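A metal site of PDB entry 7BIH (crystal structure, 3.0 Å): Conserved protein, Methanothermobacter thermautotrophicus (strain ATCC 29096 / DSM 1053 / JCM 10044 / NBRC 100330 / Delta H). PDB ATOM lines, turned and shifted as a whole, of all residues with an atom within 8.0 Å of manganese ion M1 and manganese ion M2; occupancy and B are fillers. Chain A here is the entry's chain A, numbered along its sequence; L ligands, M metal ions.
Within 4 Å of manganese ion M1: Asp 47, Asp 94, His 115 and Asp 171.
The side-chain carboxylate (OD2) of Asp 94 is bound to manganese ion M2, 2.0 Å away.
An oxygen (O1) of the ligand binds manganese ion M2, at 2.2 Å.
The side-chain carboxylate (OD2) of Asp 45 binds manganese ion M2, at 2.3 Å.
Manganese ion M2 has three donor atoms within binding distance.
Slightly farther from manganese ion M2 lies OD1 of Asp 45 (2.7 Å).
Slightly farther from manganese ion M2 lies a ring nitrogen (ND1) of His 43 (2.7 Å).
Slightly farther from manganese ion M2 lies O4 of the ligand (2.8 Å).
The backbone NH (N) of Asp 94 is in hydrogen-bond range of the backbone carbonyl oxygen (O) of Ala 113 (2.8 Å).
N of Ala 145 sits at hydrogen-bond distance from OD1 of Asp 47 (3.2 Å).
OG of Ser 144 sits at hydrogen-bond distance from OD1 of Asp 47 (2.9 Å).
The side-chain carboxylate (OD1) of Asp 47 lies within hydrogen-bond range of the backbone NH (N) of Ser 146, at 3.0 Å.
The side-chain carboxylate (OD1) of Asp 45 is in hydrogen-bond range of a ring nitrogen (ND1) of His 43 (3.1 Å).
A ring nitrogen (ND1) of His 115 lies within hydrogen-bond range of the backbone carbonyl oxygen (O) of Gly 139, 2.7 Å away.
ND1 of His 115 lies within hydrogen-bond range of O of Leu 143.
A ring nitrogen (NE2) of His 43 sits at hydrogen-bond distance from the backbone carbonyl oxygen of Ser 72 (3.1 Å).
Within 4 Å of manganese ion M2: His 43, Asp 45 and Asp 94.
The nearest printed residue that does not touch manganese ion M2 is Asp 171 (4.2 Å).
Manganese ion M1 is bound by O4 of the ligand (1.9 Å), OD1 of Asp 94 (2.1 Å), OD2 of Asp 47 (2.1 Å), OD2 of Asp 171 (2.3 Å) and NE2 of His 115 (2.5 Å).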
ATOM      1  N   SER A  42      14.374 -31.880  22.731  1.00  0.00           N
ATOM      2  CA  SER A  42      14.115 -30.646  23.446  1.00  0.00           C
ATOM      3  C   SER A  42      12.656 -30.302  23.602  1.00  0.00           C
ATOM      4  O   SER A  42      11.765 -30.985  23.095  1.00  0.00           O
ATOM      5  CB  SER A  42      14.858 -29.480  22.789  1.00  0.00           C
ATOM      6  OG  SER A  42      14.912 -28.339  23.640  1.00  0.00           O
ATOM      7  N   HIS A  43      12.451 -29.219  24.340  1.00  0.00           N
ATOM      8  CA  HIS A  43      11.117 -28.719  24.699  1.00  0.00           C
ATOM      9  C   HIS A  43      10.596 -27.776  23.622  1.00  0.00           C
ATOM     10  O   HIS A  43      11.341 -27.416  22.697  1.00  0.00           O
ATOM     11  CB  HIS A  43      11.212 -28.024  26.048  1.00  0.00           C
ATOM     12  CG  HIS A  43       9.916 -27.871  26.761  1.00  0.00           C
ATOM     13  ND1 HIS A  43       9.497 -26.670  27.272  1.00  0.00           N
ATOM     14  CD2 HIS A  43       8.949 -28.774  27.052  1.00  0.00           C
ATOM     15  CE1 HIS A  43       8.327 -26.825  27.848  1.00  0.00           C
ATOM     16  NE2 HIS A  43       7.956 -28.086  27.715  1.00  0.00           N
ATOM     17  N   ASN A  44       9.333 -27.371  23.734  1.00  0.00           N
ATOM     18  CA  ASN A  44       8.591 -26.693  22.657  1.00  0.00           C
ATOM     19  C   ASN A  44       8.245 -25.233  22.880  1.00  0.00           C
ATOM     20  O   ASN A  44       7.327 -24.713  22.263  1.00  0.00           O
ATOM     21  CB  ASN A  44       7.298 -27.451  22.389  1.00  0.00           C
ATOM     22  CG  ASN A  44       6.355 -27.420  23.559  1.00  0.00           C
ATOM     23  OD1 ASN A  44       6.735 -27.101  24.695  1.00  0.00           O
ATOM     24  ND2 ASN A  44       5.130 -27.775  23.302  1.00  0.00           N
ATOM     25  N   ASP A  45       8.969 -24.568  23.777  1.00  0.00           N
ATOM     26  CA  ASP A  45       8.807 -23.144  24.047  1.00  0.00           C
ATOM     27  C   ASP A  45      10.083 -22.396  23.588  1.00  0.00           C
ATOM     28  O   ASP A  45      10.978 -22.999  23.023  1.00  0.00           O
ATOM     29  CB  ASP A  45       8.482 -22.926  25.529  1.00  0.00           C
ATOM     30  CG  ASP A  45       9.460 -23.592  26.472  1.00  0.00           C
ATOM     31  OD1 ASP A  45      10.556 -24.011  26.058  1.00  0.00           O
ATOM     32  OD2 ASP A  45       9.139 -23.751  27.660  1.00  0.00           O
ATOM     33  N   ALA A  46      10.151 -21.087  23.809  1.00  0.00           N
ATOM     34  CA  ALA A  46      11.297 -20.306  23.360  1.00  0.00           C
ATOM     35  C   ALA A  46      12.594 -20.901  23.845  1.00  0.00           C
ATOM     36  O   ALA A  46      13.521 -21.088  23.054  1.00  0.00           O
ATOM     37  CB  ALA A  46      11.169 -18.861  23.822  1.00  0.00           C
ATOM     38  N   ASP A  47      12.674 -21.181  25.131  1.00  0.00           N
ATOM     39  CA  ASP A  47      13.883 -21.740  25.735  1.00  0.00           C
ATOM     40  C   ASP A  47      14.235 -23.087  25.107  1.00  0.00           C
ATOM     41  O   ASP A  47      15.383 -23.325  24.759  1.00  0.00           O
ATOM     42  CB  ASP A  47      13.703 -21.898  27.248  1.00  0.00           C
ATOM     43  CG  ASP A  47      14.970 -22.280  27.960  1.00  0.00           C
ATOM     44  OD1 ASP A  47      16.045 -21.783  27.572  1.00  0.00           O
ATOM     45  OD2 ASP A  47      14.885 -23.044  28.971  1.00  0.00           O
ATOM     46  N   GLY A  48      13.255 -23.945  24.930  1.00  0.00           N
ATOM     47  CA  GLY A  48      13.478 -25.255  24.370  1.00  0.00           C
ATOM     48  C   GLY A  48      13.926 -25.240  22.935  1.00  0.00           C
ATOM     49  O   GLY A  48      14.830 -25.981  22.553  1.00  0.00           O
ATOM     50  N   LEU A  49      13.286 -24.396  22.144  1.00  0.00           N
ATOM     51  CA  LEU A  49      13.656 -24.260  20.743  1.00  0.00           C
ATOM     52  C   LEU A  49      15.005 -23.541  20.544  1.00  0.00           C
ATOM     53  O   LEU A  49      15.799 -23.948  19.695  1.00  0.00           O
ATOM     54  CB  LEU A  49      12.573 -23.563  19.965  1.00  0.00           C
ATOM     55  CG  LEU A  49      11.260 -24.300  19.810  1.00  0.00           C
ATOM     56  CD1 LEU A  49      10.319 -23.403  19.021  1.00  0.00           C
ATOM     57  CD2 LEU A  49      11.401 -25.580  19.036  1.00  0.00           C
ATOM     58  N   ALA A  51      17.460 -23.496  22.766  1.00  0.00           N
ATOM     59  CA  ALA A  51      18.457 -24.475  23.211  1.00  0.00           C
ATOM     60  C   ALA A  51      18.757 -25.503  22.120  1.00  0.00           C
ATOM     61  O   ALA A  51      19.927 -25.752  21.811  1.00  0.00           O
ATOM     62  CB  ALA A  51      18.020 -25.172  24.501  1.00  0.00           C
ATOM     63  N   LEU A  71       9.416 -32.082  22.036  1.00  0.00           N
ATOM     64  CA  LEU A  71       8.328 -32.625  22.859  1.00  0.00           C
ATOM     65  C   LEU A  71       7.776 -31.562  23.784  1.00  0.00           C
ATOM     66  O   LEU A  71       8.525 -30.692  24.228  1.00  0.00           O
ATOM     67  CB  LEU A  71       8.872 -33.729  23.762  1.00  0.00           C
ATOM     68  CG  LEU A  71       9.675 -34.852  23.101  1.00  0.00           C
ATOM     69  CD1 LEU A  71      10.159 -35.772  24.202  1.00  0.00           C
ATOM     70  CD2 LEU A  71       8.850 -35.613  22.070  1.00  0.00           C
ATOM     71  N   SER A  72       6.488 -31.658  24.104  1.00  0.00           N
ATOM     72  CA  SER A  72       5.858 -30.776  25.111  1.00  0.00           C
ATOM     73  C   SER A  72       6.068 -31.272  26.544  1.00  0.00           C
ATOM     74  O   SER A  72       5.986 -30.497  27.484  1.00  0.00           O
ATOM     75  CB  SER A  72       4.379 -30.608  24.844  1.00  0.00           C
ATOM     76  OG  SER A  72       3.761 -31.856  24.743  1.00  0.00           O
ATOM     77  N   CYS A  93      17.721 -31.165  26.085  1.00  0.00           N
ATOM     78  CA  CYS A  93      17.643 -29.763  26.505  1.00  0.00           C
ATOM     79  C   CYS A  93      16.311 -29.448  27.194  1.00  0.00           C
ATOM     80  O   CYS A  93      15.243 -29.828  26.702  1.00  0.00           O
ATOM     81  CB  CYS A  93      17.782 -28.848  25.289  1.00  0.00           C
ATOM     82  SG  CYS A  93      19.213 -29.149  24.213  1.00  0.00           S
ATOM     83  N   ASP A  94      16.391 -28.736  28.310  1.00  0.00           N
ATOM     84  CA  ASP A  94      15.199 -28.197  29.020  1.00  0.00           C
ATOM     85  C   ASP A  94      14.321 -29.273  29.650  1.00  0.00           C
ATOM     86  O   ASP A  94      13.165 -29.025  29.965  1.00  0.00           O
ATOM     87  CB  ASP A  94      14.363 -27.330  28.053  1.00  0.00           C
ATOM     88  CG  ASP A  94      13.520 -26.269  28.761  1.00  0.00           C
ATOM     89  OD1 ASP A  94      13.854 -25.808  29.894  1.00  0.00           O
ATOM     90  OD2 ASP A  94      12.514 -25.869  28.150  1.00  0.00           O
ATOM     91  N   MET A  95      14.898 -30.460  29.838  1.00  0.00           N
ATOM     92  CA  MET A  95      14.213 -31.595  30.410  1.00  0.00           C
ATOM     93  C   MET A  95      15.221 -32.678  30.704  1.00  0.00           C
ATOM     94  O   MET A  95      16.368 -32.560  30.301  1.00  0.00           O
ATOM     95  CB  MET A  95      13.124 -32.131  29.483  1.00  0.00           C
ATOM     96  CG  MET A  95      13.581 -32.590  28.117  1.00  0.00           C
ATOM     97  SD  MET A  95      12.175 -32.490  26.994  1.00  0.00           S
ATOM     98  CE  MET A  95      12.780 -33.408  25.611  1.00  0.00           C
ATOM     99  N   ALA A 113      21.209 -31.082  29.381  1.00  0.00           N
ATOM    100  CA  ALA A 113      21.300 -29.661  29.627  1.00  0.00           C
ATOM    101  C   ALA A 113      19.947 -29.171  30.131  1.00  0.00           C
ATOM    102  O   ALA A 113      18.994 -29.047  29.376  1.00  0.00           O
ATOM    103  CB  ALA A 113      21.652 -28.948  28.323  1.00  0.00           C
ATOM    104  N   ASP A 114      19.851 -28.899  31.427  1.00  0.00           N
ATOM    105  CA  ASP A 114      18.552 -28.626  32.019  1.00  0.00           C
ATOM    106  C   ASP A 114      18.682 -27.693  33.213  1.00  0.00           C
ATOM    107  O   ASP A 114      19.804 -27.434  33.674  1.00  0.00           O
ATOM    108  CB  ASP A 114      17.907 -29.946  32.425  1.00  0.00           C
ATOM    109  CG  ASP A 114      16.403 -29.839  32.622  1.00  0.00           C
ATOM    110  OD1 ASP A 114      15.830 -28.757  32.342  1.00  0.00           O
ATOM    111  OD2 ASP A 114      15.821 -30.829  33.118  1.00  0.00           O
ATOM    112  N   HIS A 115      17.563 -27.144  33.675  1.00  0.00           N
ATOM    113  CA  HIS A 115      17.615 -26.191  34.783  1.00  0.00           C
ATOM    114  C   HIS A 115      16.475 -26.298  35.763  1.00  0.00           C
ATOM    115  O   HIS A 115      16.218 -25.352  36.506  1.00  0.00           O
ATOM    116  CB  HIS A 115      17.782 -24.765  34.239  1.00  0.00           C
ATOM    117  CG  HIS A 115      16.583 -24.211  33.532  1.00  0.00           C
ATOM    118  ND1 HIS A 115      16.010 -23.011  33.908  1.00  0.00           N
ATOM    119  CD2 HIS A 115      15.873 -24.646  32.453  1.00  0.00           C
ATOM    120  CE1 HIS A 115      14.994 -22.743  33.094  1.00  0.00           C
ATOM    121  NE2 HIS A 115      14.897 -23.714  32.200  1.00  0.00           N
ATOM    122  N   HIS A 116      15.821 -27.462  35.794  1.00  0.00           N
ATOM    123  CA  HIS A 116      14.831 -27.771  36.813  1.00  0.00           C
ATOM    124  C   HIS A 116      15.530 -28.389  38.034  1.00  0.00           C
ATOM    125  O   HIS A 116      16.589 -28.997  37.890  1.00  0.00           O
ATOM    126  CB  HIS A 116      13.802 -28.723  36.228  1.00  0.00           C
ATOM    127  CG  HIS A 116      13.050 -28.163  35.072  1.00  0.00           C
ATOM    128  ND1 HIS A 116      13.574 -28.119  33.802  1.00  0.00           N
ATOM    129  CD2 HIS A 116      11.812 -27.618  34.975  1.00  0.00           C
ATOM    130  CE1 HIS A 116      12.702 -27.581  32.971  1.00  0.00           C
ATOM    131  NE2 HIS A 116      11.617 -27.277  33.664  1.00  0.00           N
ATOM    132  N   GLY A 139      18.339 -22.027  38.956  1.00  0.00           N
ATOM    133  CA  GLY A 139      17.696 -22.347  37.673  1.00  0.00           C
ATOM    134  C   GLY A 139      16.469 -21.504  37.280  1.00  0.00           C
ATOM    135  O   GLY A 139      16.056 -21.488  36.127  1.00  0.00           O
ATOM    136  N   LEU A 143      20.184 -19.033  34.833  1.00  0.00           N
ATOM    137  CA  LEU A 143      20.452 -19.807  33.628  1.00  0.00           C
ATOM    138  C   LEU A 143      19.236 -20.646  33.179  1.00  0.00           C
ATOM    139  O   LEU A 143      18.464 -21.138  34.005  1.00  0.00           O
ATOM    140  CB  LEU A 143      21.639 -20.732  33.850  1.00  0.00           C
ATOM    141  CG  LEU A 143      22.290 -21.376  32.647  1.00  0.00           C
ATOM    142  CD1 LEU A 143      22.900 -20.325  31.736  1.00  0.00           C
ATOM    143  CD2 LEU A 143      23.364 -22.320  33.157  1.00  0.00           C
ATOM    144  N   SER A 144      19.056 -20.759  31.866  1.00  0.00           N
ATOM    145  CA  SER A 144      17.959 -21.504  31.267  1.00  0.00           C
ATOM    146  C   SER A 144      18.565 -22.620  30.429  1.00  0.00           C
ATOM    147  O   SER A 144      19.789 -22.760  30.399  1.00  0.00           O
ATOM    148  CB  SER A 144      17.047 -20.583  30.412  1.00  0.00           C
ATOM    149  OG  SER A 144      17.674 -20.071  29.236  1.00  0.00           O
ATOM    150  N   ALA A 145      17.736 -23.427  29.774  1.00  0.00           N
ATOM    151  CA  ALA A 145      18.225 -24.512  28.950  1.00  0.00           C
ATOM    152  C   ALA A 145      19.139 -24.028  27.814  1.00  0.00           C
ATOM    153  O   ALA A 145      20.208 -24.607  27.571  1.00  0.00           O
ATOM    154  CB  ALA A 145      17.074 -25.315  28.381  1.00  0.00           C
ATOM    155  N   SER A 146      18.721 -22.964  27.147  1.00  0.00           N
ATOM    156  CA  SER A 146      19.480 -22.408  26.036  1.00  0.00           C
ATOM    157  C   SER A 146      20.899 -21.967  26.439  1.00  0.00           C
ATOM    158  O   SER A 146      21.854 -22.295  25.742  1.00  0.00           O
ATOM    159  CB  SER A 146      18.706 -21.241  25.407  1.00  0.00           C
ATOM    160  OG  SER A 146      18.435 -20.252  26.374  1.00  0.00           O
ATOM    161  N   GLY A 167      16.394 -17.688  24.874  1.00  0.00           N
ATOM    162  CA  GLY A 167      15.749 -18.612  25.806  1.00  0.00           C
ATOM    163  C   GLY A 167      15.640 -18.057  27.219  1.00  0.00           C
ATOM    164  O   GLY A 167      14.630 -18.264  27.879  1.00  0.00           O
ATOM    165  N   ALA A 168      16.675 -17.362  27.669  1.00  0.00           N
ATOM    166  CA  ALA A 168      16.638 -16.776  29.003  1.00  0.00           C
ATOM    167  C   ALA A 168      15.497 -15.813  29.125  1.00  0.00           C
ATOM    168  O   ALA A 168      14.762 -15.822  30.122  1.00  0.00           O
ATOM    169  CB  ALA A 168      17.955 -16.081  29.354  1.00  0.00           C
ATOM    170  N   GLY A 170      12.836 -15.672  27.124  1.00  0.00           N
ATOM    171  CA  GLY A 170      11.676 -16.576  27.048  1.00  0.00           C
ATOM    172  C   GLY A 170      11.257 -17.167  28.377  1.00  0.00           C
ATOM    173  O   GLY A 170      10.102 -17.154  28.712  1.00  0.00           O
ATOM    174  N   ASP A 171      12.231 -17.610  29.161  1.00  0.00           N
ATOM    175  CA  ASP A 171      11.978 -18.162  30.498  1.00  0.00           C
ATOM    176  C   ASP A 171      11.957 -17.081  31.626  1.00  0.00           C
ATOM    177  O   ASP A 171      12.007 -17.417  32.801  1.00  0.00           O
ATOM    178  CB  ASP A 171      13.042 -19.252  30.826  1.00  0.00           C
ATOM    179  CG  ASP A 171      12.610 -20.647  30.426  1.00  0.00           C
ATOM    180  OD1 ASP A 171      11.623 -20.780  29.644  1.00  0.00           O
ATOM    181  OD2 ASP A 171      13.264 -21.615  30.897  1.00  0.00           O
ATOM    182  N   GLN A 173      13.951 -14.649  32.786  1.00  0.00           N
ATOM    183  CA  GLN A 173      15.106 -14.576  33.673  1.00  0.00           C
ATOM    184  C   GLN A 173      15.781 -13.190  33.674  1.00  0.00           C
ATOM    185  O   GLN A 173      16.828 -12.999  34.297  1.00  0.00           O
ATOM    186  CB  GLN A 173      16.106 -15.693  33.329  1.00  0.00           C
ATOM    187  CG  GLN A 173      15.525 -17.077  33.516  1.00  0.00           C
ATOM    188  CD  GLN A 173      16.543 -18.205  33.500  1.00  0.00           C
ATOM    189  OE1 GLN A 173      17.681 -18.024  33.055  1.00  0.00           O
ATOM    190  NE2 GLN A 173      16.116 -19.396  33.961  1.00  0.00           N
ATOM    191  N   ASP A 294       8.002 -18.609  20.736  1.00  0.00           N
ATOM    192  CA  ASP A 294       6.806 -19.032  21.512  1.00  0.00           C
ATOM    193  C   ASP A 294       5.631 -19.275  20.600  1.00  0.00           C
ATOM    194  O   ASP A 294       4.894 -20.242  20.812  1.00  0.00           O
ATOM    195  CB  ASP A 294       6.425 -18.029  22.591  1.00  0.00           C
ATOM    196  CG  ASP A 294       7.361 -18.084  23.797  1.00  0.00           C
ATOM    197  OD1 ASP A 294       7.696 -19.207  24.253  1.00  0.00           O
ATOM    198  OD2 ASP A 294       7.753 -16.998  24.308  1.00  0.00           O
ATOM    199  N   HIS A 427       9.121 -24.859  38.161  1.00  0.00           N
ATOM    200  CA  HIS A 427      10.050 -24.028  38.919  1.00  0.00           C
ATOM    201  C   HIS A 427       9.252 -23.370  40.053  1.00  0.00           C
ATOM    202  O   HIS A 427       8.030 -23.549  40.164  1.00  0.00           O
ATOM    203  CB  HIS A 427      10.688 -22.945  38.022  1.00  0.00           C
ATOM    204  CG  HIS A 427      11.375 -23.466  36.793  1.00  0.00           C
ATOM    205  ND1 HIS A 427      12.720 -23.771  36.745  1.00  0.00           N
ATOM    206  CD2 HIS A 427      10.913 -23.674  35.539  1.00  0.00           C
ATOM    207  CE1 HIS A 427      13.049 -24.203  35.538  1.00  0.00           C
ATOM    208  NE2 HIS A 427      11.968 -24.138  34.787  1.00  0.00           N
HETATM  209  P1  LIG L   1      10.407 -24.613  31.533  1.00  0.00           P
HETATM  210  O1  LIG L   1       9.940 -25.544  30.382  1.00  0.00           O
HETATM  211  O2  LIG L   1      10.452 -25.364  32.821  1.00  0.00           O
HETATM  212  O3  LIG L   1       9.479 -23.452  31.777  1.00  0.00           O
HETATM  213  O4  LIG L   1      11.763 -24.043  31.219  1.00  0.00           O
HETATM  214 MN    MN M   1      13.316 -23.781  30.210  1.00  0.00          MN
HETATM  215 MN    MN M   2      10.928 -24.801  28.619  1.00  0.00          MN
